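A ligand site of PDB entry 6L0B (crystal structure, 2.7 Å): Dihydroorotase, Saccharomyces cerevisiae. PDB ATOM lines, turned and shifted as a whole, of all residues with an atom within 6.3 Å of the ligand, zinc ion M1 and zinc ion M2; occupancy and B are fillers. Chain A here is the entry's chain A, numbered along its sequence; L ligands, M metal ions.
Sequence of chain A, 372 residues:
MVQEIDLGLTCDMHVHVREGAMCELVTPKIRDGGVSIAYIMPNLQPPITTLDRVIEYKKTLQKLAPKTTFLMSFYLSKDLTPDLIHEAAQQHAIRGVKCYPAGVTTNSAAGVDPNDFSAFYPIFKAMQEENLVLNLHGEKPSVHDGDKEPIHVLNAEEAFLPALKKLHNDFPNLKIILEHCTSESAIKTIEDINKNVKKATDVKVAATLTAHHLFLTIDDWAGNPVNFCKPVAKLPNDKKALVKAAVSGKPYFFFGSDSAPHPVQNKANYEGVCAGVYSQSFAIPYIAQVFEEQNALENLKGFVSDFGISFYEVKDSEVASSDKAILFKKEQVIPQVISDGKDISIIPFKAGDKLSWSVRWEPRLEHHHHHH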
ATOM      1  N   HIS A  14      -4.320  -4.784  -4.710  1.00  0.00           N
ATOM      2  CA  HIS A  14      -4.573  -5.175  -6.097  1.00  0.00           C
ATOM      3  C   HIS A  14      -3.504  -4.504  -6.960  1.00  0.00           C
ATOM      4  O   HIS A  14      -3.704  -3.395  -7.454  1.00  0.00           O
ATOM      5  CB  HIS A  14      -5.962  -4.790  -6.547  1.00  0.00           C
ATOM      6  CG  HIS A  14      -6.435  -5.524  -7.756  1.00  0.00           C
ATOM      7  ND1 HIS A  14      -7.606  -6.244  -7.777  1.00  0.00           N
ATOM      8  CD2 HIS A  14      -5.897  -5.659  -8.998  1.00  0.00           C
ATOM      9  CE1 HIS A  14      -7.783  -6.780  -8.976  1.00  0.00           C
ATOM     10  NE2 HIS A  14      -6.761  -6.432  -9.728  1.00  0.00           N
ATOM     11  N   VAL A  15      -2.398  -5.186  -7.168  1.00  0.00           N
ATOM     12  CA  VAL A  15      -1.248  -4.618  -7.847  1.00  0.00           C
ATOM     13  C   VAL A  15      -0.852  -5.545  -8.979  1.00  0.00           C
ATOM     14  O   VAL A  15      -0.912  -6.770  -8.847  1.00  0.00           O
ATOM     15  CB  VAL A  15      -0.076  -4.392  -6.882  1.00  0.00           C
ATOM     16  CG1 VAL A  15       1.133  -3.864  -7.629  1.00  0.00           C
ATOM     17  CG2 VAL A  15      -0.454  -3.455  -5.739  1.00  0.00           C
ATOM     18  N   HIS A  16      -0.512  -4.965 -10.141  1.00  0.00           N
ATOM     19  CA  HIS A  16       0.161  -5.669 -11.220  1.00  0.00           C
ATOM     20  C   HIS A  16       1.497  -4.996 -11.518  1.00  0.00           C
ATOM     21  O   HIS A  16       1.529  -3.779 -11.704  1.00  0.00           O
ATOM     22  CB  HIS A  16      -0.711  -5.725 -12.497  1.00  0.00           C
ATOM     23  CG  HIS A  16      -2.088  -6.291 -12.287  1.00  0.00           C
ATOM     24  ND1 HIS A  16      -2.519  -7.444 -12.905  1.00  0.00           N
ATOM     25  CD2 HIS A  16      -3.136  -5.845 -11.549  1.00  0.00           C
ATOM     26  CE1 HIS A  16      -3.753  -7.714 -12.528  1.00  0.00           C
ATOM     27  NE2 HIS A  16      -4.152  -6.759 -11.703  1.00  0.00           N
ATOM     28  N   ARG A  18       4.026  -6.884 -13.655  1.00  0.00           N
ATOM     29  CA  ARG A  18       4.567  -7.510 -14.875  1.00  0.00           C
ATOM     30  C   ARG A  18       5.927  -8.137 -14.562  1.00  0.00           C
ATOM     31  O   ARG A  18       6.191  -8.579 -13.443  1.00  0.00           O
ATOM     32  CB  ARG A  18       4.599  -6.500 -16.024  1.00  0.00           C
ATOM     33  CG  ARG A  18       3.388  -5.564 -16.151  1.00  0.00           C
ATOM     34  CD  ARG A  18       2.087  -6.272 -16.587  1.00  0.00           C
ATOM     35  NE  ARG A  18       0.982  -5.349 -16.900  1.00  0.00           N
ATOM     36  CZ  ARG A  18      -0.332  -5.583 -16.740  1.00  0.00           C
ATOM     37  NH1 ARG A  18      -0.818  -6.729 -16.236  1.00  0.00           N
ATOM     38  NH2 ARG A  18      -1.189  -4.621 -17.064  1.00  0.00           N
ATOM     39  N   MET A  41      -0.446  -9.603  -8.162  1.00  0.00           N
ATOM     40  CA  MET A  41      -1.378 -10.400  -8.950  1.00  0.00           C
ATOM     41  C   MET A  41      -0.654 -11.372  -9.888  1.00  0.00           C
ATOM     42  O   MET A  41       0.523 -11.172 -10.219  1.00  0.00           O
ATOM     43  CB  MET A  41      -2.312  -9.486  -9.748  1.00  0.00           C
ATOM     44  CG  MET A  41      -3.450  -8.895  -8.898  1.00  0.00           C
ATOM     45  SD  MET A  41      -4.503 -10.104  -8.047  1.00  0.00           S
ATOM     46  CE  MET A  41      -5.611  -8.992  -7.138  1.00  0.00           C
ATOM     47  N   ASN A  43      -1.320 -12.711 -13.148  1.00  0.00           N
ATOM     48  CA  ASN A  43      -1.634 -12.856 -14.572  1.00  0.00           C
ATOM     49  C   ASN A  43      -0.445 -12.463 -15.443  1.00  0.00           C
ATOM     50  O   ASN A  43      -0.489 -11.524 -16.253  1.00  0.00           O
ATOM     51  CB  ASN A  43      -2.876 -12.033 -14.897  1.00  0.00           C
ATOM     52  CG  ASN A  43      -2.633 -10.548 -14.755  1.00  0.00           C
ATOM     53  OD1 ASN A  43      -1.716 -10.147 -14.022  1.00  0.00           O
ATOM     54  ND2 ASN A  43      -3.415  -9.734 -15.469  1.00  0.00           N
ATOM     55  N   KCX A  98      -6.212 -15.706  -7.240  1.00  0.00           N
ATOM     56  CA  KCX A  98      -6.984 -14.750  -8.026  1.00  0.00           C
ATOM     57  CB  KCX A  98      -6.111 -13.597  -8.556  1.00  0.00           C
ATOM     58  CG  KCX A  98      -6.812 -12.680  -9.572  1.00  0.00           C
ATOM     59  CD  KCX A  98      -7.974 -11.949  -8.882  1.00  0.00           C
ATOM     60  CE  KCX A  98      -8.530 -10.828  -9.719  1.00  0.00           C
ATOM     61  NZ  KCX A  98      -7.329 -10.229 -10.315  1.00  0.00           N
ATOM     62  C   KCX A  98      -7.609 -15.455  -9.198  1.00  0.00           C
ATOM     63  O   KCX A  98      -6.938 -16.123  -9.982  1.00  0.00           O
ATOM     64  CX  KCX A  98      -7.343  -9.122 -11.044  1.00  0.00           C
ATOM     65  OQ1 KCX A  98      -6.278  -8.702 -11.506  1.00  0.00           O
ATOM     66  OQ2 KCX A  98      -8.392  -8.495 -11.238  1.00  0.00           O
ATOM     67  N   TYR A 100      -9.650 -15.321 -12.705  1.00  0.00           N
ATOM     68  CA  TYR A 100      -9.983 -14.550 -13.905  1.00  0.00           C
ATOM     69  C   TYR A 100     -11.008 -15.320 -14.723  1.00  0.00           C
ATOM     70  O   TYR A 100     -10.678 -16.411 -15.233  1.00  0.00           O
ATOM     71  CB  TYR A 100      -8.739 -14.272 -14.771  1.00  0.00           C
ATOM     72  CG  TYR A 100      -7.692 -13.353 -14.162  1.00  0.00           C
ATOM     73  CD1 TYR A 100      -7.774 -11.962 -14.266  1.00  0.00           C
ATOM     74  CD2 TYR A 100      -6.608 -13.892 -13.476  1.00  0.00           C
ATOM     75  CE1 TYR A 100      -6.806 -11.129 -13.703  1.00  0.00           C
ATOM     76  CE2 TYR A 100      -5.640 -13.073 -12.909  1.00  0.00           C
ATOM     77  CZ  TYR A 100      -5.727 -11.707 -13.026  1.00  0.00           C
ATOM     78  OH  TYR A 100      -4.747 -10.949 -12.439  1.00  0.00           O
ATOM     79  N   THR A 105     -10.369 -10.042 -19.514  1.00  0.00           N
ATOM     80  CA  THR A 105      -9.368  -9.009 -19.270  1.00  0.00           C
ATOM     81  C   THR A 105      -7.998  -9.521 -19.703  1.00  0.00           C
ATOM     82  O   THR A 105      -7.876 -10.614 -20.266  1.00  0.00           O
ATOM     83  CB  THR A 105      -9.381  -8.617 -17.782  1.00  0.00           C
ATOM     84  OG1 THR A 105      -8.431  -7.582 -17.553  1.00  0.00           O
ATOM     85  CG2 THR A 105      -9.026  -9.832 -16.928  1.00  0.00           C
ATOM     86  N   THR A 106      -6.946  -8.773 -19.353  1.00  0.00           N
ATOM     87  CA  THR A 106      -5.574  -9.079 -19.781  1.00  0.00           C
ATOM     88  C   THR A 106      -5.116 -10.418 -19.231  1.00  0.00           C
ATOM     89  O   THR A 106      -5.231 -10.669 -18.032  1.00  0.00           O
ATOM     90  CB  THR A 106      -4.604  -8.012 -19.273  1.00  0.00           C
ATOM     91  OG1 THR A 106      -4.905  -6.732 -19.831  1.00  0.00           O
ATOM     92  CG2 THR A 106      -3.174  -8.374 -19.613  1.00  0.00           C
ATOM     93  N   ASN A 107      -4.551 -11.259 -20.106  1.00  0.00           N
ATOM     94  CA  ASN A 107      -3.983 -12.540 -19.700  1.00  0.00           C
ATOM     95  C   ASN A 107      -4.997 -13.368 -18.908  1.00  0.00           C
ATOM     96  O   ASN A 107      -4.702 -13.856 -17.822  1.00  0.00           O
ATOM     97  CB  ASN A 107      -2.682 -12.350 -18.905  1.00  0.00           C
ATOM     98  CG  ASN A 107      -1.534 -11.848 -19.777  1.00  0.00           C
ATOM     99  OD1 ASN A 107      -1.652 -11.792 -21.007  1.00  0.00           O
ATOM    100  ND2 ASN A 107      -0.402 -11.500 -19.146  1.00  0.00           N
ATOM    101  N   HIS A 137     -12.225 -11.472  -9.911  1.00  0.00           N
ATOM    102  CA  HIS A 137     -12.579 -10.523 -10.969  1.00  0.00           C
ATOM    103  C   HIS A 137     -13.990 -10.863 -11.416  1.00  0.00           C
ATOM    104  O   HIS A 137     -14.188 -11.628 -12.346  1.00  0.00           O
ATOM    105  CB  HIS A 137     -11.616 -10.582 -12.145  1.00  0.00           C
ATOM    106  CG  HIS A 137     -11.914  -9.572 -13.222  1.00  0.00           C
ATOM    107  ND1 HIS A 137     -11.016  -8.597 -13.595  1.00  0.00           N
ATOM    108  CD2 HIS A 137     -13.007  -9.399 -14.014  1.00  0.00           C
ATOM    109  CE1 HIS A 137     -11.529  -7.869 -14.566  1.00  0.00           C
ATOM    110  NE2 HIS A 137     -12.736  -8.343 -14.843  1.00  0.00           N
ATOM    111  N   GLU A 179     -13.142  -7.994  -6.281  1.00  0.00           N
ATOM    112  CA  GLU A 179     -12.152  -7.004  -6.686  1.00  0.00           C
ATOM    113  C   GLU A 179     -12.754  -5.901  -7.535  1.00  0.00           C
ATOM    114  O   GLU A 179     -13.678  -6.136  -8.333  1.00  0.00           O
ATOM    115  CB  GLU A 179     -11.008  -7.654  -7.486  1.00  0.00           C
ATOM    116  CG  GLU A 179     -10.211  -8.655  -6.704  1.00  0.00           C
ATOM    117  CD  GLU A 179      -9.243  -8.007  -5.737  1.00  0.00           C
ATOM    118  OE1 GLU A 179      -8.829  -6.850  -5.953  1.00  0.00           O
ATOM    119  OE2 GLU A 179      -8.893  -8.682  -4.753  1.00  0.00           O
ATOM    120  N   HIS A 180     -12.140  -4.715  -7.434  1.00  0.00           N
ATOM    121  CA  HIS A 180     -12.497  -3.495  -8.163  1.00  0.00           C
ATOM    122  C   HIS A 180     -13.986  -3.377  -8.480  1.00  0.00           C
ATOM    123  O   HIS A 180     -14.384  -3.499  -9.649  1.00  0.00           O
ATOM    124  CB  HIS A 180     -11.663  -3.376  -9.461  1.00  0.00           C
ATOM    125  CG  HIS A 180     -11.489  -4.657 -10.235  1.00  0.00           C
ATOM    126  ND1 HIS A 180     -12.511  -5.569 -10.410  1.00  0.00           N
ATOM    127  CD2 HIS A 180     -10.430  -5.129 -10.936  1.00  0.00           C
ATOM    128  CE1 HIS A 180     -12.065  -6.578 -11.140  1.00  0.00           C
ATOM    129  NE2 HIS A 180     -10.814  -6.333 -11.472  1.00  0.00           N
ATOM    130  N   CYS A 229     -10.428   0.142 -19.077  1.00  0.00           N
ATOM    131  CA  CYS A 229      -9.995  -0.902 -18.162  1.00  0.00           C
ATOM    132  C   CYS A 229     -11.145  -1.890 -17.984  1.00  0.00           C
ATOM    133  O   CYS A 229     -12.266  -1.658 -18.446  1.00  0.00           O
ATOM    134  CB  CYS A 229      -9.532  -0.311 -16.831  1.00  0.00           C
ATOM    135  SG  CYS A 229     -10.873   0.261 -15.767  1.00  0.00           S
ATOM    136  N   LYS A 230     -10.866  -3.004 -17.293  1.00  0.00           N
ATOM    137  CA  LYS A 230     -11.925  -3.960 -16.975  1.00  0.00           C
ATOM    138  C   LYS A 230     -11.993  -4.118 -15.458  1.00  0.00           C
ATOM    139  O   LYS A 230     -10.935  -4.163 -14.815  1.00  0.00           O
ATOM    140  CB  LYS A 230     -11.687  -5.322 -17.647  1.00  0.00           C
ATOM    141  CG  LYS A 230     -11.687  -5.301 -19.178  1.00  0.00           C
ATOM    142  CD  LYS A 230     -12.974  -4.736 -19.727  1.00  0.00           C
ATOM    143  CE  LYS A 230     -14.149  -5.679 -19.544  1.00  0.00           C
ATOM    144  NZ  LYS A 230     -14.184  -6.738 -20.597  1.00  0.00           N
ATOM    145  N   PRO A 231     -13.188  -4.064 -14.833  1.00  0.00           N
ATOM    146  CA  PRO A 231     -14.465  -3.756 -15.494  1.00  0.00           C
ATOM    147  C   PRO A 231     -14.499  -2.286 -15.906  1.00  0.00           C
ATOM    148  O   PRO A 231     -13.855  -1.452 -15.263  1.00  0.00           O
ATOM    149  CB  PRO A 231     -15.513  -4.043 -14.425  1.00  0.00           C
ATOM    150  CG  PRO A 231     -14.815  -4.852 -13.388  1.00  0.00           C
ATOM    151  CD  PRO A 231     -13.372  -4.460 -13.432  1.00  0.00           C
ATOM    152  N   ASP A 258      -5.524  -1.839  -8.617  1.00  0.00           N
ATOM    153  CA  ASP A 258      -5.438  -2.463  -9.941  1.00  0.00           C
ATOM    154  C   ASP A 258      -4.667  -1.568 -10.906  1.00  0.00           C
ATOM    155  O   ASP A 258      -5.048  -1.361 -12.053  1.00  0.00           O
ATOM    156  CB  ASP A 258      -6.825  -2.795 -10.496  1.00  0.00           C
ATOM    157  CG  ASP A 258      -6.778  -3.561 -11.828  1.00  0.00           C
ATOM    158  OD1 ASP A 258      -5.747  -4.208 -12.145  1.00  0.00           O
ATOM    159  OD2 ASP A 258      -7.782  -3.544 -12.552  1.00  0.00           O
ATOM    160  N   SER A 259      -3.566  -1.011 -10.424  1.00  0.00           N
ATOM    161  CA  SER A 259      -2.687  -0.349 -11.364  1.00  0.00           C
ATOM    162  C   SER A 259      -2.175  -1.415 -12.314  1.00  0.00           C
ATOM    163  O   SER A 259      -1.538  -2.381 -11.882  1.00  0.00           O
ATOM    164  CB  SER A 259      -1.580   0.384 -10.607  1.00  0.00           C
ATOM    165  OG  SER A 259      -0.690   1.054 -11.493  1.00  0.00           O
ATOM    166  N   ALA A 260      -2.513  -1.291 -13.607  1.00  0.00           N
ATOM    167  CA  ALA A 260      -2.192  -2.289 -14.641  1.00  0.00           C
ATOM    168  C   ALA A 260      -1.404  -1.620 -15.770  1.00  0.00           C
ATOM    169  O   ALA A 260      -1.982  -1.111 -16.734  1.00  0.00           O
ATOM    170  CB  ALA A 260      -3.464  -2.936 -15.178  1.00  0.00           C
ATOM    171  N   PRO A 261      -0.070  -1.628 -15.687  1.00  0.00           N
ATOM    172  CA  PRO A 261       0.740  -0.925 -16.689  1.00  0.00           C
ATOM    173  C   PRO A 261       0.804  -1.667 -18.015  1.00  0.00           C
ATOM    174  O   PRO A 261       0.780  -2.898 -18.045  1.00  0.00           O
ATOM    175  CB  PRO A 261       2.118  -0.801 -16.007  1.00  0.00           C
ATOM    176  CG  PRO A 261       2.147  -1.921 -14.996  1.00  0.00           C
ATOM    177  CD  PRO A 261       0.733  -2.173 -14.571  1.00  0.00           C
ATOM    178  N   HIS A 262       0.794  -0.908 -19.115  1.00  0.00           N
ATOM    179  CA  HIS A 262       1.016  -1.373 -20.505  1.00  0.00           C
ATOM    180  C   HIS A 262       1.823  -0.299 -21.217  1.00  0.00           C
ATOM    181  O   HIS A 262       1.609   0.899 -20.970  1.00  0.00           O
ATOM    182  CB  HIS A 262      -0.272  -1.615 -21.306  1.00  0.00           C
ATOM    183  CG  HIS A 262      -1.273  -2.484 -20.613  1.00  0.00           C
ATOM    184  ND1 HIS A 262      -1.506  -3.793 -21.001  1.00  0.00           N
ATOM    185  CD2 HIS A 262      -2.152  -2.224 -19.616  1.00  0.00           C
ATOM    186  CE1 HIS A 262      -2.445  -4.312 -20.236  1.00  0.00           C
ATOM    187  NE2 HIS A 262      -2.849  -3.381 -19.387  1.00  0.00           N
ATOM    188  N   CYS A 274      -5.372  -2.765 -25.080  1.00  0.00           N
ATOM    189  CA  CYS A 274      -5.150  -3.470 -23.819  1.00  0.00           C
ATOM    190  C   CYS A 274      -5.894  -2.783 -22.685  1.00  0.00           C
ATOM    191  O   CYS A 274      -5.796  -1.561 -22.504  1.00  0.00           O
ATOM    192  CB  CYS A 274      -3.662  -3.524 -23.506  1.00  0.00           C
ATOM    193  SG  CYS A 274      -2.683  -4.419 -24.687  1.00  0.00           S
ATOM    194  N   ALA A 275      -6.637  -3.558 -21.900  1.00  0.00           N
ATOM    195  CA  ALA A 275      -7.297  -3.025 -20.720  1.00  0.00           C
ATOM    196  C   ALA A 275      -6.284  -2.723 -19.625  1.00  0.00           C
ATOM    197  O   ALA A 275      -5.319  -3.467 -19.426  1.00  0.00           O
ATOM    198  CB  ALA A 275      -8.340  -4.018 -20.214  1.00  0.00           C
ATOM    199  N   GLY A 276      -6.511  -1.627 -18.886  1.00  0.00           N
ATOM    200  CA  GLY A 276      -5.655  -1.302 -17.749  1.00  0.00           C
ATOM    201  C   GLY A 276      -5.266   0.153 -17.563  1.00  0.00           C
ATOM    202  O   GLY A 276      -4.792   0.836 -18.484  1.00  0.00           O
ATOM    203  N   VAL A 277      -5.424   0.633 -16.337  1.00  0.00           N
ATOM    204  CA  VAL A 277      -5.052   1.995 -16.000  1.00  0.00           C
ATOM    205  C   VAL A 277      -3.881   1.931 -15.054  1.00  0.00           C
ATOM    206  O   VAL A 277      -3.934   1.222 -14.036  1.00  0.00           O
ATOM    207  CB  VAL A 277      -6.232   2.754 -15.369  1.00  0.00           C
ATOM    208  CG1 VAL A 277      -5.757   4.081 -14.843  1.00  0.00           C
ATOM    209  CG2 VAL A 277      -7.341   2.952 -16.396  1.00  0.00           C
HETATM  210  N1  LIG L   1      -7.184  -5.280 -16.251  1.00  0.00           N
HETATM  211  C1  LIG L   1      -7.013  -6.274 -15.162  1.00  0.00           C
HETATM  212  N2  LIG L   1      -5.669  -6.912 -15.050  1.00  0.00           N
HETATM  213  C2  LIG L   1      -4.588  -6.549 -15.974  1.00  0.00           C
HETATM  214  C3  LIG L   1      -4.793  -5.573 -17.046  1.00  0.00           C
HETATM  215  C4  LIG L   1      -6.096  -4.971 -17.152  1.00  0.00           C
HETATM  216  O1  LIG L   1      -7.921  -6.559 -14.422  1.00  0.00           O
HETATM  217  O2  LIG L   1      -3.495  -7.002 -15.923  1.00  0.00           O
HETATM  218  F1  LIG L   1      -3.711  -5.325 -17.876  1.00  0.00           F
HETATM  219 ZN    ZN M   1      -6.246  -6.478 -11.898  1.00  0.00          ZN
HETATM  220 ZN    ZN M   2      -9.383  -7.571 -12.868  1.00  0.00          ZN
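A ring nitrogen (NE2) of His 16 is bound to zinc ion M1 (2.1 Å). Zinc ion M1 is bound by a ring nitrogen (NE2) of His 14, 2.2 Å away. Zinc ion M1 is bound by OQ1 of KCX 98, at 2.3 Å. OD1 of Asp 258 binds zinc ion M1, 2.3 Å away.
NZ of KCX 98 sits at hydrogen-bond distance from the side-chain sulfur (SD) of Met 41, 3.6 Å away. The backbone NH of His 16 is in hydrogen-bond range of the backbone carbonyl oxygen of Ser 259, 3.3 Å away. A ring nitrogen (NE2) of His 262 lies within hydrogen-bond range of the guanidinium group (NH2) of Arg 18 (3.1 Å). NE2 of His 262 sits at hydrogen-bond distance from O of Ala 275 (2.5 Å). O of Thr 106 sits at hydrogen-bond distance from ND2 of Asn 43 (3.3 Å). O of Ala 275 sits at hydrogen-bond distance from OG1 of Thr 106, 3.3 Å away. The guanidinium group of Arg 18 lies within hydrogen-bond range of the backbone carbonyl oxygen of Pro 261 (2.7 Å). N of Ala 260 is in hydrogen-bond range of O of Val 277 (2.9 Å).
Within 4 Å of zinc ion M1: His 14, His 16, KCX 98 and Asp 258.
The side-chain hydroxyl (OG1) of Thr 106 sits close to a fluorine (F1) of the ligand (2.7 Å). NE2 of His 262 sits close to F1 of the ligand. The backbone carbonyl oxygen (O) of Ala 275 lies close to a fluorine (F1) of the ligand, 2.9 Å away. Lys 230 touches the ligand (O to O1, 3.9 Å). Ala 260 touches the ligand. Gly 276 touches the ligand (CA to C4, 3.7 Å). Along chain A the residues within 4 Å of the ligand span positions 16 to 276. The nearest printed residue that does not touch the ligand is His 180 (4.1 Å).
Zinc ion M2 is bound by ND1 of His 137 (2.1 Å), OQ2 of KCX 98 (2.1 Å), NE2 of His 180 (2.4 Å) and O1 of the ligand (2.4 Å). Zinc ion M2 has four donor atoms within binding distance.
ND1 of His 16 lies within hydrogen-bond range of O2 of the ligand, 3.2 Å away. NH1 of Arg 18 is in hydrogen-bond range of O2 of the ligand, 2.7 Å away. O2 of the ligand is in hydrogen-bond range of ND2 of Asn 43 (2.8 Å). N1 of the ligand lies within hydrogen-bond range of OG1 of Thr 105 (2.9 Å).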
